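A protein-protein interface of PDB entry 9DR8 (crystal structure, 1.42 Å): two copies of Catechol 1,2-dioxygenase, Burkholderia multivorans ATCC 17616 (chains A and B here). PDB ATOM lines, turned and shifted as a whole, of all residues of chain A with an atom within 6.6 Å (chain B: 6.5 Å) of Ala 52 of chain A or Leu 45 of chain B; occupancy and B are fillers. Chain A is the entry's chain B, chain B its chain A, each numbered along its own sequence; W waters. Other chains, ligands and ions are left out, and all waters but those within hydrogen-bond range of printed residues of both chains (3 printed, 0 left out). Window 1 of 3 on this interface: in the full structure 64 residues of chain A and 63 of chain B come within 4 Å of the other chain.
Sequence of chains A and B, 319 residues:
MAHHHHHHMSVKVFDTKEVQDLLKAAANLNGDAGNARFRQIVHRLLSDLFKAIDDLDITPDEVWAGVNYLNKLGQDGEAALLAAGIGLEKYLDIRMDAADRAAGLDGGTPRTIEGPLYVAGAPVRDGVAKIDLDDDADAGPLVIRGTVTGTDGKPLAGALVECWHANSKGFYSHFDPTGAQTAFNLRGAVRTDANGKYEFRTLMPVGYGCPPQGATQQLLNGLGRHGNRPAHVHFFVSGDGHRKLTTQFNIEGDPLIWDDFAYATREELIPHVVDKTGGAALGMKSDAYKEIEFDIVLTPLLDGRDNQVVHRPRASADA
The side-chain hydroxyl (OH) of Tyr 91 of chain B is in hydrogen-bond range of the backbone carbonyl oxygen (O) of Phe 50 of chain A, at 2.7 Å.
The side-chain carboxylate of Asp 55 of chain A lies within salt-bridge range of the guanidinium group of Arg 44 of chain B (2.9 Å).
The side-chain carboxylate of Asp 55 of chain A lies within salt-bridge range of the side-chain amino group of Lys 51 of chain A, at 3.9 Å.
The guanidinium group (NE) of Arg 44 of chain B is in salt-bridge range of the side-chain carboxylate (OD2) of Asp 48 of chain B (2.9 Å).
N of Phe 14 of chain A lies within hydrogen-bond range of OD2 of Asp 54 of chain A (3.1 Å).
O of Ile 53 of chain A lies within hydrogen-bond range of N of Ile 58 of chain A (3.0 Å).
OD2 of Asp 48 of chain B touches O of Asp 48 of chain A, 3.9 Å away.
CG of Lys 51 of chain A touches NH2 of Arg 44 of chain B, 3.9 Å away.
Ala 52 of chain A touches Arg 44 of chain B (CA to NH2, 3.7 Å).
CD2 of Leu 45 of chain B touches CB of Ala 52 of chain A (3.97 Å).
Ile 53 of chain A touches Tyr 91 of chain B.
CB of Asp 54 of chain A touches OH of Tyr 91 of chain B, 3.4 Å away.
Gln 40 of chain B touches Leu 56 of chain A.
Arg 44 of chain B touches Leu 56 of chain A.
Ser 47 of chain A touches none of the printed residues of chain B.
Printed residues of chain B within 4 Å of Asp 48 of chain A: Asp 48 (3.9 Å).
Of the printed residues of chain B, Lys 51 of chain A touches Arg 44 (3.9 Å).
Of the printed residues of chain B, Ala 52 of chain A touches Arg 44 (3.7 Å) and Leu 45 (3.97 Å).
Of the printed residues of chain B, Asp 54 of chain A touches Tyr 91 (3.4 Å).
Ile 58 of chain A touches none of the printed residues of chain B.
Leu 45 of chain B touches just one residue of chain A: Ala 52.
The nearest residue of chain A that does not touch Leu 45 of chain B is Leu 49 of chain A (4.2 Å).
Of the 13 printed residues of chain A, 8 touch a printed residue of chain B.
Among the printed residues, Asp or Glu carboxylates within 4 Å of a Lys or Arg side-chain nitrogen of the other chain: Asp 55 of chain A with Arg 44 of chain B.
Asp 48 of chain A touches its own counterpart, Asp 48 of chain B.
Positions printed for both chains: 47, 48, 49 and 50.
Water W3 lies within hydrogen-bond range of OD2 of Asp 48 of chain B (2.6 Å), O of Asp 48 of chain A (2.7 Å) and NH2 of Arg 44 of chain B (2.9 Å).
Water W1 lies within hydrogen-bond range of the side-chain carboxylate of Asp 48 of chain A and the backbone carbonyl oxygen of Asp 48 of chain B.
Water W2 bridges OD2 of Asp 48 of chain B and O of Asp 48 of chain A.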
ATOM      1  N   PHE A  14      36.023   1.085  31.665  1.00  0.00           N
ATOM      2  CA  PHE A  14      35.609   2.282  32.391  1.00  0.00           C
ATOM      3  C   PHE A  14      35.767   2.098  33.889  1.00  0.00           C
ATOM      4  O   PHE A  14      36.267   2.991  34.585  1.00  0.00           O
ATOM      5  CB  PHE A  14      34.166   2.656  32.061  1.00  0.00           C
ATOM      6  CG  PHE A  14      33.661   3.826  32.856  1.00  0.00           C
ATOM      7  CD1 PHE A  14      33.994   5.119  32.495  1.00  0.00           C
ATOM      8  CD2 PHE A  14      32.887   3.629  33.984  1.00  0.00           C
ATOM      9  CE1 PHE A  14      33.542   6.194  33.223  1.00  0.00           C
ATOM     10  CE2 PHE A  14      32.415   4.702  34.715  1.00  0.00           C
ATOM     11  CZ  PHE A  14      32.750   5.986  34.339  1.00  0.00           C
ATOM     12  N   SER A  47      33.060  11.718  32.990  1.00  0.00           N
ATOM     13  CA  SER A  47      32.792  10.329  33.344  1.00  0.00           C
ATOM     14  C   SER A  47      31.704   9.750  32.453  1.00  0.00           C
ATOM     15  O   SER A  47      31.834   8.641  31.934  1.00  0.00           O
ATOM     16  CB  SER A  47      32.376  10.235  34.812  1.00  0.00           C
ATOM     17  OG  SER A  47      33.428  10.607  35.683  1.00  0.00           O
ATOM     18  N   ASP A  48      30.611  10.494  32.265  1.00  0.00           N
ATOM     19  CA  ASP A  48      29.544   9.990  31.406  1.00  0.00           C
ATOM     20  C   ASP A  48      30.035   9.797  29.977  1.00  0.00           C
ATOM     21  O   ASP A  48      29.681   8.813  29.322  1.00  0.00           O
ATOM     22  CB  ASP A  48      28.335  10.921  31.419  1.00  0.00           C
ATOM     23  CG  ASP A  48      27.591  10.915  32.742  1.00  0.00           C
ATOM     24  OD1 ASP A  48      27.744   9.969  33.538  1.00  0.00           O
ATOM     25  OD2 ASP A  48      26.818  11.864  32.967  1.00  0.00           O
ATOM     26  N   LEU A  49      30.859  10.721  29.480  1.00  0.00           N
ATOM     27  CA  LEU A  49      31.384  10.580  28.126  1.00  0.00           C
ATOM     28  C   LEU A  49      32.267   9.346  28.010  1.00  0.00           C
ATOM     29  O   LEU A  49      32.140   8.567  27.059  1.00  0.00           O
ATOM     30  CB  LEU A  49      32.161  11.836  27.739  1.00  0.00           C
ATOM     31  CG  LEU A  49      32.930  11.760  26.424  1.00  0.00           C
ATOM     32  CD1 LEU A  49      31.985  11.575  25.239  1.00  0.00           C
ATOM     33  CD2 LEU A  49      33.797  13.012  26.266  1.00  0.00           C
ATOM     34  N   PHE A  50      33.179   9.156  28.966  1.00  0.00           N
ATOM     35  CA  PHE A  50      34.058   7.993  28.926  1.00  0.00           C
ATOM     36  C   PHE A  50      33.240   6.708  29.001  1.00  0.00           C
ATOM     37  O   PHE A  50      33.538   5.728  28.311  1.00  0.00           O
ATOM     38  CB  PHE A  50      35.044   8.035  30.100  1.00  0.00           C
ATOM     39  CG  PHE A  50      36.199   8.991  29.933  1.00  0.00           C
ATOM     40  CD1 PHE A  50      36.118  10.100  29.107  1.00  0.00           C
ATOM     41  CD2 PHE A  50      37.374   8.775  30.634  1.00  0.00           C
ATOM     42  CE1 PHE A  50      37.184  10.973  28.992  1.00  0.00           C
ATOM     43  CE2 PHE A  50      38.434   9.641  30.516  1.00  0.00           C
ATOM     44  CZ  PHE A  50      38.342  10.737  29.692  1.00  0.00           C
ATOM     45  N   LYS A  51      32.199   6.691  29.833  1.00  0.00           N
ATOM     46  CA  LYS A  51      31.381   5.490  29.963  1.00  0.00           C
ATOM     47  C   LYS A  51      30.608   5.218  28.680  1.00  0.00           C
ATOM     48  O   LYS A  51      30.438   4.063  28.287  1.00  0.00           O
ATOM     49  CB  LYS A  51      30.434   5.626  31.158  1.00  0.00           C
ATOM     50  CG  LYS A  51      29.491   4.444  31.374  1.00  0.00           C
ATOM     51  CD  LYS A  51      30.229   3.193  31.816  1.00  0.00           C
ATOM     52  CE  LYS A  51      29.259   2.086  32.203  1.00  0.00           C
ATOM     53  NZ  LYS A  51      29.969   0.917  32.791  1.00  0.00           N
ATOM     54  N   ALA A  52      30.129   6.276  28.011  1.00  0.00           N
ATOM     55  CA  ALA A  52      29.418   6.079  26.751  1.00  0.00           C
ATOM     56  C   ALA A  52      30.345   5.545  25.670  1.00  0.00           C
ATOM     57  O   ALA A  52      29.956   4.681  24.875  1.00  0.00           O
ATOM     58  CB  ALA A  52      28.781   7.392  26.294  1.00  0.00           C
ATOM     59  N   ILE A  53      31.572   6.064  25.610  1.00  0.00           N
ATOM     60  CA  ILE A  53      32.556   5.544  24.666  1.00  0.00           C
ATOM     61  C   ILE A  53      32.794   4.059  24.913  1.00  0.00           C
ATOM     62  O   ILE A  53      32.881   3.256  23.972  1.00  0.00           O
ATOM     63  CB  ILE A  53      33.855   6.362  24.773  1.00  0.00           C
ATOM     64  CG1 ILE A  53      33.647   7.756  24.180  1.00  0.00           C
ATOM     65  CG2 ILE A  53      35.002   5.618  24.102  1.00  0.00           C
ATOM     66  CD1 ILE A  53      34.784   8.715  24.487  1.00  0.00           C
ATOM     67  N   ASP A  54      32.882   3.669  26.184  1.00  0.00           N
ATOM     68  CA  ASP A  54      33.140   2.276  26.543  1.00  0.00           C
ATOM     69  C   ASP A  54      31.933   1.400  26.219  1.00  0.00           C
ATOM     70  O   ASP A  54      32.084   0.306  25.662  1.00  0.00           O
ATOM     71  CB  ASP A  54      33.476   2.229  28.043  1.00  0.00           C
ATOM     72  CG  ASP A  54      34.309   1.019  28.458  1.00  0.00           C
ATOM     73  OD1 ASP A  54      35.328   0.694  27.810  1.00  0.00           O
ATOM     74  OD2 ASP A  54      33.958   0.411  29.490  1.00  0.00           O
ATOM     75  N   ASP A  55      30.722   1.886  26.522  1.00  0.00           N
ATOM     76  CA  ASP A  55      29.521   1.069  26.367  1.00  0.00           C
ATOM     77  C   ASP A  55      29.166   0.867  24.901  1.00  0.00           C
ATOM     78  O   ASP A  55      28.715  -0.214  24.512  1.00  0.00           O
ATOM     79  CB  ASP A  55      28.337   1.741  27.059  1.00  0.00           C
ATOM     80  CG  ASP A  55      28.292   1.494  28.553  1.00  0.00           C
ATOM     81  OD1 ASP A  55      29.030   0.621  29.056  1.00  0.00           O
ATOM     82  OD2 ASP A  55      27.487   2.181  29.226  1.00  0.00           O
ATOM     83  N   LEU A  56      29.310   1.910  24.088  1.00  0.00           N
ATOM     84  CA  LEU A  56      28.966   1.854  22.675  1.00  0.00           C
ATOM     85  C   LEU A  56      30.163   1.533  21.794  1.00  0.00           C
ATOM     86  O   LEU A  56      30.027   1.526  20.567  1.00  0.00           O
ATOM     87  CB  LEU A  56      28.348   3.185  22.223  1.00  0.00           C
ATOM     88  CG  LEU A  56      26.982   3.532  22.821  1.00  0.00           C
ATOM     89  CD1 LEU A  56      26.475   4.860  22.283  1.00  0.00           C
ATOM     90  CD2 LEU A  56      25.989   2.411  22.540  1.00  0.00           C
ATOM     91  N   ASP A  57      31.323   1.255  22.394  1.00  0.00           N
ATOM     92  CA  ASP A  57      32.565   1.007  21.665  1.00  0.00           C
ATOM     93  C   ASP A  57      32.791   2.073  20.595  1.00  0.00           C
ATOM     94  O   ASP A  57      33.013   1.783  19.418  1.00  0.00           O
ATOM     95  CB  ASP A  57      32.615  -0.403  21.073  1.00  0.00           C
ATOM     96  CG  ASP A  57      34.038  -0.841  20.724  1.00  0.00           C
ATOM     97  OD1 ASP A  57      35.003  -0.261  21.270  1.00  0.00           O
ATOM     98  OD2 ASP A  57      34.193  -1.766  19.902  1.00  0.00           O
ATOM     99  N   ILE A  58      32.721   3.330  21.016  1.00  0.00           N
ATOM    100  CA  ILE A  58      32.951   4.426  20.084  1.00  0.00           C
ATOM    101  C   ILE A  58      34.430   4.437  19.724  1.00  0.00           C
ATOM    102  O   ILE A  58      35.298   4.466  20.607  1.00  0.00           O
ATOM    103  CB  ILE A  58      32.477   5.759  20.683  1.00  0.00           C
ATOM    104  CG1 ILE A  58      31.007   5.647  21.124  1.00  0.00           C
ATOM    105  CG2 ILE A  58      32.632   6.878  19.659  1.00  0.00           C
ATOM    106  CD1 ILE A  58      30.410   6.945  21.674  1.00  0.00           C
ATOM    107  N   GLN B  40      22.055   6.503  17.425  1.00  0.00           N
ATOM    108  CA  GLN B  40      22.322   5.818  18.687  1.00  0.00           C
ATOM    109  C   GLN B  40      23.286   6.621  19.547  1.00  0.00           C
ATOM    110  O   GLN B  40      23.060   6.806  20.749  1.00  0.00           O
ATOM    111  CB  GLN B  40      22.898   4.422  18.394  1.00  0.00           C
ATOM    112  CG  GLN B  40      23.361   3.618  19.619  1.00  0.00           C
ATOM    113  CD  GLN B  40      24.286   2.442  19.264  1.00  0.00           C
ATOM    114  OE1 GLN B  40      25.026   2.481  18.274  1.00  0.00           O
ATOM    115  NE2 GLN B  40      24.249   1.396  20.083  1.00  0.00           N
ATOM    116  N   ILE B  41      24.378   7.098  18.945  1.00  0.00           N
ATOM    117  CA  ILE B  41      25.358   7.880  19.696  1.00  0.00           C
ATOM    118  C   ILE B  41      24.737   9.178  20.195  1.00  0.00           C
ATOM    119  O   ILE B  41      24.885   9.540  21.369  1.00  0.00           O
ATOM    120  CB  ILE B  41      26.619   8.131  18.849  1.00  0.00           C
ATOM    121  CG1 ILE B  41      27.382   6.817  18.660  1.00  0.00           C
ATOM    122  CG2 ILE B  41      27.517   9.166  19.504  1.00  0.00           C
ATOM    123  CD1 ILE B  41      28.497   6.904  17.655  1.00  0.00           C
ATOM    124  N   VAL B  42      24.041   9.904  19.314  1.00  0.00           N
ATOM    125  CA  VAL B  42      23.455  11.182  19.714  1.00  0.00           C
ATOM    126  C   VAL B  42      22.442  10.984  20.833  1.00  0.00           C
ATOM    127  O   VAL B  42      22.427  11.735  21.813  1.00  0.00           O
ATOM    128  CB  VAL B  42      22.843  11.906  18.497  1.00  0.00           C
ATOM    129  CG1 VAL B  42      22.005  13.101  18.940  1.00  0.00           C
ATOM    130  CG2 VAL B  42      23.945  12.369  17.549  1.00  0.00           C
ATOM    131  N   HIS B  43      21.584   9.968  20.719  1.00  0.00           N
ATOM    132  CA  HIS B  43      20.605   9.737  21.773  1.00  0.00           C
ATOM    133  C   HIS B  43      21.286   9.448  23.103  1.00  0.00           C
ATOM    134  O   HIS B  43      20.860   9.950  24.144  1.00  0.00           O
ATOM    135  CB  HIS B  43      19.649   8.605  21.411  1.00  0.00           C
ATOM    136  CG  HIS B  43      18.561   8.393  22.421  1.00  0.00           C
ATOM    137  ND1 HIS B  43      18.628   7.416  23.392  1.00  0.00           N
ATOM    138  CD2 HIS B  43      17.387   9.039  22.616  1.00  0.00           C
ATOM    139  CE1 HIS B  43      17.533   7.459  24.133  1.00  0.00           C
ATOM    140  NE2 HIS B  43      16.766   8.438  23.685  1.00  0.00           N
ATOM    141  N   ARG B  44      22.359   8.656  23.090  1.00  0.00           N
ATOM    142  CA  ARG B  44      23.045   8.313  24.332  1.00  0.00           C
ATOM    143  C   ARG B  44      23.681   9.547  24.954  1.00  0.00           C
ATOM    144  O   ARG B  44      23.542   9.792  26.156  1.00  0.00           O
ATOM    145  CB  ARG B  44      24.104   7.243  24.060  1.00  0.00           C
ATOM    146  CG  ARG B  44      25.035   6.935  25.243  1.00  0.00           C
ATOM    147  CD  ARG B  44      24.273   6.520  26.500  1.00  0.00           C
ATOM    148  NE  ARG B  44      25.189   6.218  27.594  1.00  0.00           N
ATOM    149  CZ  ARG B  44      25.693   5.022  27.853  1.00  0.00           C
ATOM    150  NH1 ARG B  44      25.324   3.950  27.171  1.00  0.00           N
ATOM    151  NH2 ARG B  44      26.615   4.903  28.800  1.00  0.00           N
ATOM    152  N   LEU B  45      24.372  10.349  24.147  1.00  0.00           N
ATOM    153  CA  LEU B  45      25.037  11.525  24.694  1.00  0.00           C
ATOM    154  C   LEU B  45      24.026  12.555  25.190  1.00  0.00           C
ATOM    155  O   LEU B  45      24.222  13.176  26.243  1.00  0.00           O
ATOM    156  CB  LEU B  45      25.961  12.127  23.637  1.00  0.00           C
ATOM    157  CG  LEU B  45      27.136  11.231  23.246  1.00  0.00           C
ATOM    158  CD1 LEU B  45      28.033  11.913  22.222  1.00  0.00           C
ATOM    159  CD2 LEU B  45      27.952  10.820  24.471  1.00  0.00           C
ATOM    160  N   LEU B  46      22.935  12.744  24.452  1.00  0.00           N
ATOM    161  CA  LEU B  46      21.908  13.685  24.879  1.00  0.00           C
ATOM    162  C   LEU B  46      21.217  13.204  26.150  1.00  0.00           C
ATOM    163  O   LEU B  46      20.978  13.994  27.074  1.00  0.00           O
ATOM    164  CB  LEU B  46      20.900  13.868  23.745  1.00  0.00           C
ATOM    165  CG  LEU B  46      19.929  15.038  23.841  1.00  0.00           C
ATOM    166  CD1 LEU B  46      20.672  16.362  23.856  1.00  0.00           C
ATOM    167  CD2 LEU B  46      18.966  14.976  22.669  1.00  0.00           C
ATOM    168  N   SER B  47      20.883  11.912  26.210  1.00  0.00           N
ATOM    169  CA  SER B  47      20.239  11.375  27.399  1.00  0.00           C
ATOM    170  C   SER B  47      21.144  11.529  28.613  1.00  0.00           C
ATOM    171  O   SER B  47      20.697  11.948  29.686  1.00  0.00           O
ATOM    172  CB  SER B  47      19.880   9.908  27.163  1.00  0.00           C
ATOM    173  OG  SER B  47      19.303   9.328  28.314  1.00  0.00           O
ATOM    174  N   ASP B  48      22.427  11.223  28.453  1.00  0.00           N
ATOM    175  CA  ASP B  48      23.353  11.374  29.565  1.00  0.00           C
ATOM    176  C   ASP B  48      23.446  12.832  30.004  1.00  0.00           C
ATOM    177  O   ASP B  48      23.473  13.123  31.203  1.00  0.00           O
ATOM    178  CB  ASP B  48      24.733  10.853  29.168  1.00  0.00           C
ATOM    179  CG  ASP B  48      24.811   9.331  29.117  1.00  0.00           C
ATOM    180  OD1 ASP B  48      23.905   8.638  29.627  1.00  0.00           O
ATOM    181  OD2 ASP B  48      25.815   8.826  28.581  1.00  0.00           O
ATOM    182  N   LEU B  49      23.504  13.762  29.042  1.00  0.00           N
ATOM    183  CA  LEU B  49      23.561  15.182  29.380  1.00  0.00           C
ATOM    184  C   LEU B  49      22.323  15.608  30.157  1.00  0.00           C
ATOM    185  O   LEU B  49      22.430  16.285  31.188  1.00  0.00           O
ATOM    186  CB  LEU B  49      23.700  16.019  28.105  1.00  0.00           C
ATOM    187  CG  LEU B  49      23.669  17.536  28.303  1.00  0.00           C
ATOM    188  CD1 LEU B  49      24.801  18.002  29.206  1.00  0.00           C
ATOM    189  CD2 LEU B  49      23.701  18.262  26.967  1.00  0.00           C
ATOM    190  N   PHE B  50      21.136  15.223  29.675  1.00  0.00           N
ATOM    191  CA  PHE B  50      19.901  15.599  30.357  1.00  0.00           C
ATOM    192  C   PHE B  50      19.853  15.007  31.762  1.00  0.00           C
ATOM    193  O   PHE B  50      19.396  15.661  32.705  1.00  0.00           O
ATOM    194  CB  PHE B  50      18.671  15.126  29.573  1.00  0.00           C
ATOM    195  CG  PHE B  50      18.335  15.945  28.324  1.00  0.00           C
ATOM    196  CD1 PHE B  50      19.276  16.730  27.677  1.00  0.00           C
ATOM    197  CD2 PHE B  50      17.048  15.901  27.804  1.00  0.00           C
ATOM    198  CE1 PHE B  50      18.948  17.441  26.540  1.00  0.00           C
ATOM    199  CE2 PHE B  50      16.711  16.613  26.656  1.00  0.00           C
ATOM    200  CZ  PHE B  50      17.664  17.382  26.030  1.00  0.00           C
ATOM    201  N   TYR B  91      42.581   8.375  27.205  1.00  0.00           N
ATOM    202  CA  TYR B  91      41.583   7.327  27.375  1.00  0.00           C
ATOM    203  C   TYR B  91      41.476   6.457  26.128  1.00  0.00           C
ATOM    204  O   TYR B  91      41.326   5.234  26.228  1.00  0.00           O
ATOM    205  CB  TYR B  91      40.240   7.970  27.703  1.00  0.00           C
ATOM    206  CG  TYR B  91      39.111   7.017  27.988  1.00  0.00           C
ATOM    207  CD1 TYR B  91      39.197   6.091  29.017  1.00  0.00           C
ATOM    208  CD2 TYR B  91      37.939   7.079  27.264  1.00  0.00           C
ATOM    209  CE1 TYR B  91      38.154   5.238  29.296  1.00  0.00           C
ATOM    210  CE2 TYR B  91      36.889   6.236  27.535  1.00  0.00           C
ATOM    211  CZ  TYR B  91      36.999   5.320  28.553  1.00  0.00           C
ATOM    212  OH  TYR B  91      35.940   4.492  28.823  1.00  0.00           O
HETATM  213  O   HOH W   1      24.265  11.253  33.018  1.00  0.00           O
HETATM  214  O   HOH W   2      27.805  10.825  27.680  1.00  0.00           O
HETATM  215  O   HOH W   3      27.474   7.412  29.994  1.00  0.00           O
